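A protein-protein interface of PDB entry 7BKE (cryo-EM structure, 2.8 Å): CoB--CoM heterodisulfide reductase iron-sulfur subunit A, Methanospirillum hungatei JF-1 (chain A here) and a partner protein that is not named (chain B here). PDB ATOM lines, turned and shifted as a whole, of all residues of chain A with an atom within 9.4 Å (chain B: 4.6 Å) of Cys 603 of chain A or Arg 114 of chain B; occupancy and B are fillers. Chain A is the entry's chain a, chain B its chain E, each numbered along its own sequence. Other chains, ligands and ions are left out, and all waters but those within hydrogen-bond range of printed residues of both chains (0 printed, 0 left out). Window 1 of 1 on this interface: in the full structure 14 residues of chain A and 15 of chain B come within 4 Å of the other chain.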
ATOM      1  N   CYS A 595      25.030 -17.438  10.540  1.00  0.00           N
ATOM      2  CA  CYS A 595      23.955 -17.087  11.453  1.00  0.00           C
ATOM      3  C   CYS A 595      24.464 -16.154  12.537  1.00  0.00           C
ATOM      4  O   CYS A 595      25.491 -16.420  13.165  1.00  0.00           O
ATOM      5  CB  CYS A 595      23.356 -18.335  12.092  1.00  0.00           C
ATOM      6  SG  CYS A 595      22.069 -17.993  13.307  1.00  0.00           S
ATOM      7  N   LEU A 599      20.708 -12.647  17.190  1.00  0.00           N
ATOM      8  CA  LEU A 599      19.497 -12.257  16.492  1.00  0.00           C
ATOM      9  C   LEU A 599      18.609 -13.439  16.146  1.00  0.00           C
ATOM     10  O   LEU A 599      17.429 -13.232  15.858  1.00  0.00           O
ATOM     11  CB  LEU A 599      19.833 -11.514  15.197  1.00  0.00           C
ATOM     12  CG  LEU A 599      20.535 -10.169  15.267  1.00  0.00           C
ATOM     13  CD1 LEU A 599      20.825  -9.698  13.874  1.00  0.00           C
ATOM     14  CD2 LEU A 599      19.671  -9.168  15.974  1.00  0.00           C
ATOM     15  N   CYS A 600      19.140 -14.655  16.140  1.00  0.00           N
ATOM     16  CA  CYS A 600      18.297 -15.813  15.881  1.00  0.00           C
ATOM     17  C   CYS A 600      17.348 -16.067  17.039  1.00  0.00           C
ATOM     18  O   CYS A 600      17.732 -16.005  18.205  1.00  0.00           O
ATOM     19  CB  CYS A 600      19.140 -17.056  15.640  1.00  0.00           C
ATOM     20  SG  CYS A 600      18.182 -18.523  15.291  1.00  0.00           S
ATOM     21  N   ALA A 601      16.094 -16.366  16.709  1.00  0.00           N
ATOM     22  CA  ALA A 601      15.069 -16.672  17.688  1.00  0.00           C
ATOM     23  C   ALA A 601      14.769 -18.156  17.787  1.00  0.00           C
ATOM     24  O   ALA A 601      13.919 -18.547  18.584  1.00  0.00           O
ATOM     25  CB  ALA A 601      13.787 -15.917  17.363  1.00  0.00           C
ATOM     26  N   GLY A 602      15.435 -18.988  17.001  1.00  0.00           N
ATOM     27  CA  GLY A 602      15.266 -20.416  17.133  1.00  0.00           C
ATOM     28  C   GLY A 602      13.980 -20.974  16.594  1.00  0.00           C
ATOM     29  O   GLY A 602      13.583 -22.064  16.990  1.00  0.00           O
ATOM     30  N   CYS A 603      13.312 -20.265  15.690  1.00  0.00           N
ATOM     31  CA  CYS A 603      12.053 -20.764  15.156  1.00  0.00           C
ATOM     32  C   CYS A 603      12.245 -22.037  14.342  1.00  0.00           C
ATOM     33  O   CYS A 603      11.330 -22.858  14.265  1.00  0.00           O
ATOM     34  CB  CYS A 603      11.374 -19.686  14.317  1.00  0.00           C
ATOM     35  SG  CYS A 603      12.186 -19.256  12.791  1.00  0.00           S
ATOM     36  N   GLY A 604      13.407 -22.217  13.733  1.00  0.00           N
ATOM     37  CA  GLY A 604      13.670 -23.414  12.965  1.00  0.00           C
ATOM     38  C   GLY A 604      12.997 -23.479  11.621  1.00  0.00           C
ATOM     39  O   GLY A 604      12.998 -24.541  10.997  1.00  0.00           O
ATOM     40  N   MET A 605      12.415 -22.379  11.157  1.00  0.00           N
ATOM     41  CA  MET A 605      11.675 -22.396   9.906  1.00  0.00           C
ATOM     42  C   MET A 605      12.588 -22.376   8.691  1.00  0.00           C
ATOM     43  O   MET A 605      12.218 -22.906   7.641  1.00  0.00           O
ATOM     44  CB  MET A 605      10.695 -21.223   9.877  1.00  0.00           C
ATOM     45  CG  MET A 605       9.539 -21.400  10.845  1.00  0.00           C
ATOM     46  SD  MET A 605       8.205 -20.203  10.709  1.00  0.00           S
ATOM     47  CE  MET A 605       9.089 -18.706  10.341  1.00  0.00           C
ATOM     48  N   CYS A 606      13.778 -21.793   8.816  1.00  0.00           N
ATOM     49  CA  CYS A 606      14.743 -21.779   7.726  1.00  0.00           C
ATOM     50  C   CYS A 606      15.329 -23.148   7.436  1.00  0.00           C
ATOM     51  O   CYS A 606      15.867 -23.354   6.350  1.00  0.00           O
ATOM     52  CB  CYS A 606      15.878 -20.824   8.060  1.00  0.00           C
ATOM     53  SG  CYS A 606      16.704 -21.223   9.603  1.00  0.00           S
ATOM     54  N   VAL A 607      15.238 -24.082   8.378  1.00  0.00           N
ATOM     55  CA  VAL A 607      15.959 -25.346   8.255  1.00  0.00           C
ATOM     56  C   VAL A 607      15.528 -26.108   7.008  1.00  0.00           C
ATOM     57  O   VAL A 607      16.349 -26.740   6.337  1.00  0.00           O
ATOM     58  CB  VAL A 607      15.774 -26.177   9.532  1.00  0.00           C
ATOM     59  CG1 VAL A 607      16.191 -27.591   9.303  1.00  0.00           C
ATOM     60  CG2 VAL A 607      16.587 -25.583  10.641  1.00  0.00           C
ATOM     61  N   ASN A 608      14.250 -26.052   6.671  1.00  0.00           N
ATOM     62  CA  ASN A 608      13.736 -26.793   5.530  1.00  0.00           C
ATOM     63  C   ASN A 608      13.904 -26.061   4.212  1.00  0.00           C
ATOM     64  O   ASN A 608      13.515 -26.595   3.176  1.00  0.00           O
ATOM     65  CB  ASN A 608      12.265 -27.110   5.741  1.00  0.00           C
ATOM     66  CG  ASN A 608      12.015 -27.784   7.055  1.00  0.00           C
ATOM     67  OD1 ASN A 608      11.720 -27.131   8.051  1.00  0.00           O
ATOM     68  ND2 ASN A 608      12.151 -29.100   7.077  1.00  0.00           N
ATOM     69  N   SER A 616      20.632 -26.376  10.673  1.00  0.00           N
ATOM     70  CA  SER A 616      20.085 -27.202  11.733  1.00  0.00           C
ATOM     71  C   SER A 616      19.953 -26.347  12.981  1.00  0.00           C
ATOM     72  O   SER A 616      20.540 -25.271  13.079  1.00  0.00           O
ATOM     73  CB  SER A 616      20.959 -28.421  12.007  1.00  0.00           C
ATOM     74  OG  SER A 616      22.151 -28.046  12.667  1.00  0.00           O
ATOM     75  N   LEU A 617      19.165 -26.839  13.927  1.00  0.00           N
ATOM     76  CA  LEU A 617      18.969 -26.165  15.201  1.00  0.00           C
ATOM     77  C   LEU A 617      19.899 -26.777  16.235  1.00  0.00           C
ATOM     78  O   LEU A 617      19.941 -27.998  16.392  1.00  0.00           O
ATOM     79  CB  LEU A 617      17.518 -26.273  15.663  1.00  0.00           C
ATOM     80  CG  LEU A 617      16.562 -25.210  15.141  1.00  0.00           C
ATOM     81  CD1 LEU A 617      15.183 -25.487  15.657  1.00  0.00           C
ATOM     82  CD2 LEU A 617      17.018 -23.851  15.566  1.00  0.00           C
ATOM     83  N   GLY A 618      20.644 -25.926  16.934  1.00  0.00           N
ATOM     84  CA  GLY A 618      21.598 -26.396  17.908  1.00  0.00           C
ATOM     85  C   GLY A 618      21.616 -25.508  19.136  1.00  0.00           C
ATOM     86  O   GLY A 618      21.030 -24.429  19.160  1.00  0.00           O
ATOM     87  N   ARG A 623      20.394 -20.845  24.628  1.00  0.00           N
ATOM     88  CA  ARG A 623      19.446 -20.546  23.568  1.00  0.00           C
ATOM     89  C   ARG A 623      19.573 -21.558  22.445  1.00  0.00           C
ATOM     90  O   ARG A 623      20.675 -21.953  22.067  1.00  0.00           O
ATOM     91  CB  ARG A 623      19.684 -19.147  23.019  1.00  0.00           C
ATOM     92  CG  ARG A 623      19.814 -18.095  24.073  1.00  0.00           C
ATOM     93  CD  ARG A 623      20.262 -16.792  23.470  1.00  0.00           C
ATOM     94  NE  ARG A 623      19.254 -16.250  22.570  1.00  0.00           N
ATOM     95  CZ  ARG A 623      19.453 -16.025  21.279  1.00  0.00           C
ATOM     96  NH1 ARG A 623      20.627 -16.290  20.733  1.00  0.00           N
ATOM     97  NH2 ARG A 623      18.479 -15.531  20.536  1.00  0.00           N
ATOM     98  N   THR A 624      18.432 -21.980  21.911  1.00  0.00           N
ATOM     99  CA  THR A 624      18.412 -22.793  20.703  1.00  0.00           C
ATOM    100  C   THR A 624      18.497 -21.860  19.510  1.00  0.00           C
ATOM    101  O   THR A 624      17.578 -21.079  19.260  1.00  0.00           O
ATOM    102  CB  THR A 624      17.147 -23.639  20.643  1.00  0.00           C
ATOM    103  OG1 THR A 624      17.187 -24.631  21.674  1.00  0.00           O
ATOM    104  CG2 THR A 624      17.046 -24.327  19.307  1.00  0.00           C
ATOM    105  N   VAL A 625      19.602 -21.922  18.777  1.00  0.00           N
ATOM    106  CA  VAL A 625      19.788 -21.089  17.598  1.00  0.00           C
ATOM    107  C   VAL A 625      20.097 -21.987  16.414  1.00  0.00           C
ATOM    108  O   VAL A 625      20.243 -23.200  16.563  1.00  0.00           O
ATOM    109  CB  VAL A 625      20.902 -20.053  17.808  1.00  0.00           C
ATOM    110  CG1 VAL A 625      20.543 -19.113  18.915  1.00  0.00           C
ATOM    111  CG2 VAL A 625      22.196 -20.744  18.116  1.00  0.00           C
ATOM    112  N   MET A 626      20.202 -21.395  15.233  1.00  0.00           N
ATOM    113  CA  MET A 626      20.477 -22.139  14.017  1.00  0.00           C
ATOM    114  C   MET A 626      21.985 -22.258  13.814  1.00  0.00           C
ATOM    115  O   MET A 626      22.752 -21.375  14.196  1.00  0.00           O
ATOM    116  CB  MET A 626      19.811 -21.453  12.827  1.00  0.00           C
ATOM    117  CG  MET A 626      20.071 -22.068  11.480  1.00  0.00           C
ATOM    118  SD  MET A 626      21.539 -21.412  10.685  1.00  0.00           S
ATOM    119  CE  MET A 626      20.915 -19.965   9.870  1.00  0.00           C
ATOM    120  N   CYS A 639      17.855 -19.151   2.488  1.00  0.00           N
ATOM    121  CA  CYS A 639      17.607 -19.002   3.915  1.00  0.00           C
ATOM    122  C   CYS A 639      17.706 -17.546   4.343  1.00  0.00           C
ATOM    123  O   CYS A 639      16.864 -17.049   5.101  1.00  0.00           O
ATOM    124  CB  CYS A 639      18.598 -19.853   4.696  1.00  0.00           C
ATOM    125  SG  CYS A 639      20.326 -19.503   4.328  1.00  0.00           S
ATOM    126  N   PHE A 642      14.882 -15.556   3.384  1.00  0.00           N
ATOM    127  CA  PHE A 642      13.678 -15.878   4.136  1.00  0.00           C
ATOM    128  C   PHE A 642      13.649 -15.219   5.510  1.00  0.00           C
ATOM    129  O   PHE A 642      12.697 -14.507   5.833  1.00  0.00           O
ATOM    130  CB  PHE A 642      13.536 -17.383   4.307  1.00  0.00           C
ATOM    131  CG  PHE A 642      12.499 -17.763   5.303  1.00  0.00           C
ATOM    132  CD1 PHE A 642      11.164 -17.605   5.018  1.00  0.00           C
ATOM    133  CD2 PHE A 642      12.853 -18.242   6.537  1.00  0.00           C
ATOM    134  CE1 PHE A 642      10.209 -17.934   5.936  1.00  0.00           C
ATOM    135  CE2 PHE A 642      11.896 -18.577   7.453  1.00  0.00           C
ATOM    136  CZ  PHE A 642      10.576 -18.424   7.149  1.00  0.00           C
ATOM    137  N   CYS A 643      14.672 -15.465   6.331  1.00  0.00           N
ATOM    138  CA  CYS A 643      14.655 -15.155   7.758  1.00  0.00           C
ATOM    139  C   CYS A 643      14.089 -13.774   8.055  1.00  0.00           C
ATOM    140  O   CYS A 643      14.693 -12.764   7.682  1.00  0.00           O
ATOM    141  CB  CYS A 643      16.058 -15.260   8.347  1.00  0.00           C
ATOM    142  SG  CYS A 643      16.114 -15.025  10.125  1.00  0.00           S
ATOM    143  N   PRO A 644      12.919 -13.673   8.743  1.00  0.00           N
ATOM    144  CA  PRO A 644      12.278 -12.391   8.952  1.00  0.00           C
ATOM    145  C   PRO A 644      13.093 -11.464   9.839  1.00  0.00           C
ATOM    146  O   PRO A 644      13.071 -10.306   9.587  1.00  0.00           O
ATOM    147  CB  PRO A 644      10.939 -12.740   9.570  1.00  0.00           C
ATOM    148  CG  PRO A 644      10.726 -14.178   9.247  1.00  0.00           C
ATOM    149  CD  PRO A 644      12.114 -14.748   9.362  1.00  0.00           C
ATOM    150  N   GLY A 645      13.827 -12.001  10.815  1.00  0.00           N
ATOM    151  CA  GLY A 645      14.558 -11.177  11.742  1.00  0.00           C
ATOM    152  C   GLY A 645      15.911 -10.718  11.274  1.00  0.00           C
ATOM    153  O   GLY A 645      16.576  -9.968  11.986  1.00  0.00           O
ATOM    154  N   ALA A 647      18.595 -12.636  10.832  1.00  0.00           N
ATOM    155  CA  ALA A 647      19.584 -13.339  11.627  1.00  0.00           C
ATOM    156  C   ALA A 647      20.515 -14.188  10.792  1.00  0.00           C
ATOM    157  O   ALA A 647      21.376 -14.864  11.352  1.00  0.00           O
ATOM    158  CB  ALA A 647      18.896 -14.221  12.660  1.00  0.00           C
ATOM    159  N   ILE A 648      20.355 -14.192   9.477  1.00  0.00           N
ATOM    160  CA  ILE A 648      21.250 -14.898   8.572  1.00  0.00           C
ATOM    161  C   ILE A 648      21.958 -13.870   7.714  1.00  0.00           C
ATOM    162  O   ILE A 648      21.312 -13.074   7.029  1.00  0.00           O
ATOM    163  CB  ILE A 648      20.498 -15.911   7.699  1.00  0.00           C
ATOM    164  CG1 ILE A 648      19.638 -16.810   8.562  1.00  0.00           C
ATOM    165  CG2 ILE A 648      21.470 -16.740   6.918  1.00  0.00           C
ATOM    166  CD1 ILE A 648      18.962 -17.877   7.802  1.00  0.00           C
ATOM    167  N   GLU B 110      -0.131 -20.500  16.074  1.00  0.00           N
ATOM    168  CA  GLU B 110       0.864 -19.731  15.329  1.00  0.00           C
ATOM    169  C   GLU B 110       2.209 -19.725  16.044  1.00  0.00           C
ATOM    170  O   GLU B 110       3.262 -19.946  15.429  1.00  0.00           O
ATOM    171  CB  GLU B 110       0.369 -18.305  15.111  1.00  0.00           C
ATOM    172  CG  GLU B 110      -0.713 -18.183  14.066  1.00  0.00           C
ATOM    173  CD  GLU B 110      -0.385 -18.926  12.794  1.00  0.00           C
ATOM    174  OE1 GLU B 110       0.670 -18.657  12.192  1.00  0.00           O
ATOM    175  OE2 GLU B 110      -1.181 -19.788  12.386  1.00  0.00           O
ATOM    176  N   LEU B 111       2.199 -19.485  17.353  1.00  0.00           N
ATOM    177  CA  LEU B 111       3.454 -19.476  18.089  1.00  0.00           C
ATOM    178  C   LEU B 111       4.068 -20.868  18.181  1.00  0.00           C
ATOM    179  O   LEU B 111       5.293 -20.999  18.197  1.00  0.00           O
ATOM    180  CB  LEU B 111       3.241 -18.883  19.475  1.00  0.00           C
ATOM    181  CG  LEU B 111       3.005 -17.377  19.501  1.00  0.00           C
ATOM    182  CD1 LEU B 111       2.155 -17.004  20.669  1.00  0.00           C
ATOM    183  CD2 LEU B 111       4.310 -16.644  19.568  1.00  0.00           C
ATOM    184  N   ALA B 112       3.257 -21.918  18.222  1.00  0.00           N
ATOM    185  CA  ALA B 112       3.834 -23.254  18.213  1.00  0.00           C
ATOM    186  C   ALA B 112       4.413 -23.620  16.851  1.00  0.00           C
ATOM    187  O   ALA B 112       5.411 -24.340  16.789  1.00  0.00           O
ATOM    188  CB  ALA B 112       2.797 -24.276  18.642  1.00  0.00           C
ATOM    189  N   LYS B 113       3.796 -23.170  15.757  1.00  0.00           N
ATOM    190  CA  LYS B 113       4.425 -23.302  14.444  1.00  0.00           C
ATOM    191  C   LYS B 113       5.803 -22.672  14.451  1.00  0.00           C
ATOM    192  O   LYS B 113       6.777 -23.269  13.990  1.00  0.00           O
ATOM    193  CB  LYS B 113       3.591 -22.620  13.366  1.00  0.00           C
ATOM    194  CG  LYS B 113       2.380 -23.337  12.894  1.00  0.00           C
ATOM    195  CD  LYS B 113       1.646 -22.418  11.951  1.00  0.00           C
ATOM    196  CE  LYS B 113       0.207 -22.803  11.808  1.00  0.00           C
ATOM    197  NZ  LYS B 113      -0.593 -21.713  11.213  1.00  0.00           N
ATOM    198  N   ARG B 114       5.895 -21.447  14.950  1.00  0.00           N
ATOM    199  CA  ARG B 114       7.181 -20.771  14.978  1.00  0.00           C
ATOM    200  C   ARG B 114       8.028 -21.148  16.172  1.00  0.00           C
ATOM    201  O   ARG B 114       8.990 -20.439  16.460  1.00  0.00           O
ATOM    202  CB  ARG B 114       6.983 -19.265  14.953  1.00  0.00           C
ATOM    203  CG  ARG B 114       6.572 -18.760  13.620  1.00  0.00           C
ATOM    204  CD  ARG B 114       5.776 -17.503  13.751  1.00  0.00           C
ATOM    205  NE  ARG B 114       5.315 -17.046  12.455  1.00  0.00           N
ATOM    206  CZ  ARG B 114       4.275 -17.559  11.824  1.00  0.00           C
ATOM    207  NH1 ARG B 114       3.585 -18.540  12.371  1.00  0.00           N
ATOM    208  NH2 ARG B 114       3.927 -17.086  10.647  1.00  0.00           N
ATOM    209  N   ASN B 115       7.663 -22.197  16.904  1.00  0.00           N
ATOM    210  CA  ASN B 115       8.540 -22.823  17.890  1.00  0.00           C
ATOM    211  C   ASN B 115       8.744 -21.962  19.125  1.00  0.00           C
ATOM    212  O   ASN B 115       9.776 -22.053  19.780  1.00  0.00           O
ATOM    213  CB  ASN B 115       9.891 -23.170  17.273  1.00  0.00           C
ATOM    214  CG  ASN B 115      10.452 -24.449  17.794  1.00  0.00           C
ATOM    215  OD1 ASN B 115       9.720 -25.323  18.231  1.00  0.00           O
ATOM    216  ND2 ASN B 115      11.767 -24.575  17.747  1.00  0.00           N
ATOM    217  N   GLN B 116       7.768 -21.132  19.471  1.00  0.00           N
ATOM    218  CA  GLN B 116       7.915 -20.210  20.584  1.00  0.00           C
ATOM    219  C   GLN B 116       7.224 -20.676  21.854  1.00  0.00           C
ATOM    220  O   GLN B 116       7.455 -20.084  22.910  1.00  0.00           O
ATOM    221  CB  GLN B 116       7.387 -18.832  20.200  1.00  0.00           C
ATOM    222  CG  GLN B 116       8.005 -18.275  18.954  1.00  0.00           C
ATOM    223  CD  GLN B 116       9.469 -17.984  19.118  1.00  0.00           C
ATOM    224  OE1 GLN B 116       9.858 -17.151  19.928  1.00  0.00           O
ATOM    225  NE2 GLN B 116      10.295 -18.665  18.351  1.00  0.00           N
ATOM    226  N   ILE B 305       2.356 -13.191  15.751  1.00  0.00           N
ATOM    227  CA  ILE B 305       3.179 -13.727  14.634  1.00  0.00           C
ATOM    228  C   ILE B 305       4.529 -13.040  14.611  1.00  0.00           C
ATOM    229  O   ILE B 305       5.449 -13.549  14.003  1.00  0.00           O
ATOM    230  CB  ILE B 305       2.361 -13.657  13.326  1.00  0.00           C
ATOM    231  CG1 ILE B 305       1.310 -14.765  13.282  1.00  0.00           C
ATOM    232  CG2 ILE B 305       3.229 -13.675  12.080  1.00  0.00           C
ATOM    233  CD1 ILE B 305      -0.026 -14.357  13.824  1.00  0.00           C
ATOM    234  N   TYR B 307       7.690 -12.676  16.196  1.00  0.00           N
ATOM    235  CA  TYR B 307       8.491 -13.387  17.215  1.00  0.00           C
ATOM    236  C   TYR B 307       9.959 -13.091  17.061  1.00  0.00           C
ATOM    237  O   TYR B 307      10.727 -13.782  17.696  1.00  0.00           O
ATOM    238  CB  TYR B 307       8.505 -14.869  16.873  1.00  0.00           C
ATOM    239  CG  TYR B 307       9.151 -15.241  15.563  1.00  0.00           C
ATOM    240  CD1 TYR B 307      10.362 -15.901  15.540  1.00  0.00           C
ATOM    241  CD2 TYR B 307       8.556 -14.940  14.353  1.00  0.00           C
ATOM    242  CE1 TYR B 307      10.984 -16.220  14.351  1.00  0.00           C
ATOM    243  CE2 TYR B 307       9.156 -15.266  13.151  1.00  0.00           C
ATOM    244  CZ  TYR B 307      10.374 -15.912  13.155  1.00  0.00           C
ATOM    245  OH  TYR B 307      10.981 -16.250  11.986  1.00  0.00           O
ATOM    246  N   SER B 341      -0.155 -15.125   7.563  1.00  0.00           N
ATOM    247  CA  SER B 341      -0.802 -15.777   8.701  1.00  0.00           C
ATOM    248  C   SER B 341      -1.167 -14.722   9.738  1.00  0.00           C
ATOM    249  O   SER B 341      -0.420 -14.495  10.684  1.00  0.00           O
ATOM    250  CB  SER B 341       0.099 -16.843   9.290  1.00  0.00           C
ATOM    251  OG  SER B 341       1.359 -16.301   9.611  1.00  0.00           O
ATOM    252  N   PRO B 384       4.224 -22.304   7.912  1.00  0.00           N
ATOM    253  CA  PRO B 384       3.894 -21.138   7.093  1.00  0.00           C
ATOM    254  C   PRO B 384       4.276 -21.330   5.632  1.00  0.00           C
ATOM    255  O   PRO B 384       5.129 -22.151   5.273  1.00  0.00           O
ATOM    256  CB  PRO B 384       4.708 -20.017   7.739  1.00  0.00           C
ATOM    257  CG  PRO B 384       4.868 -20.447   9.132  1.00  0.00           C
ATOM    258  CD  PRO B 384       4.978 -21.929   9.115  1.00  0.00           C
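Printed residues of chain B that touch a printed residue of chain A: Arg 114, Asn 115, Gln 116, Tyr 307 and Pro 384.
Hydrophobic or aromatic side chains of chain B that line the printed part of chain A: Tyr 307 and Pro 384.
Printed residues of chain A that touch a printed residue of chain B: Ala 601, Gly 602, Cys 603, Met 605 and Pro 644.
Hydrophobic or aromatic side chains of chain A within 4 Å of the printed part of chain B: Ala 601, Met 605 and Pro 644.
Among the printed residues, 10 pairs touch across the chains.
The side-chain amide nitrogen (ND2) of Asn 115 of chain B lies within hydrogen-bond range of the backbone carbonyl oxygen (O) of Gly 602 of chain A (3.2 Å).
The side-chain hydroxyl of Tyr 307 of chain B lies close to the side-chain sulfur of Cys 603 of chain A, 3.3 Å away.
The side-chain sulfur (SG) of Cys 600 of chain A sits close to the backbone NH (N) of Gly 602 of chain A.
The side-chain sulfur (SG) of Cys 603 of chain A sits close to the backbone NH (N) of Met 605 of chain A (3.5 Å).
The side-chain carboxylate of Glu 110 of chain B lies within salt-bridge range of the guanidinium group of Arg 114 of chain B.
O of Leu 111 of chain B is in hydrogen-bond range of N of Gln 116 of chain B (2.8 Å).
O of Arg 114 of chain B is in hydrogen-bond range of NE2 of Gln 116 of chain B (2.9 Å).
NH2 of Arg 114 of chain B lies within hydrogen-bond range of OG of Ser 341 of chain B, at 2.9 Å.
Among the printed residues, pairs that only touch across the chains: Ala 601 of chain A with Gln 116 of chain B (3.6 Å), Ala 601 of chain A with Tyr 307 of chain B (3.7 Å), Cys 603 of chain A with Arg 114 of chain B (3.3 Å), Cys 603 of chain A with Asn 115 of chain B (3.3 Å), Met 605 of chain A with Arg 114 of chain B (3.6 Å), Met 605 of chain A with Tyr 307 of chain B (3.5 Å), Met 605 of chain A with Pro 384 of chain B (3.7 Å) and Pro 644 of chain A with Tyr 307 of chain B (3.2 Å).
Leu 599 of chain A touches none of the printed residues of chain B.
Printed residues of chain B within 4 Å of Ala 601 of chain A: Gln 116 and Tyr 307.
Cys 603 of chain A touches just these residues of chain B: Arg 114, Asn 115 and Tyr 307.
Of the printed residues of chain B, Met 605 of chain A touches Arg 114 (3.6 Å), Tyr 307 (3.5 Å) and Pro 384 (3.7 Å).
Leu 111 of chain B touches none of the printed residues of chain A.
Of chain A, only Cys 603 (3.3 Å) and Met 605 (3.6 Å) come within 4 Å of Arg 114 of chain B.
Of chain A, only Gly 602 and Cys 603 come within 4 Å of Asn 115 of chain B.
The nearest residue of chain B that does not touch Cys 603 of chain A is Gln 116 of chain B (4.2 Å).
The nearest residue of chain A that does not touch Arg 114 of chain B is Gly 602 of chain A (4.9 Å).
The nearest printed residue of chain B that does not touch Ala 601 of chain A is Asn 115 of chain B (5.6 Å).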
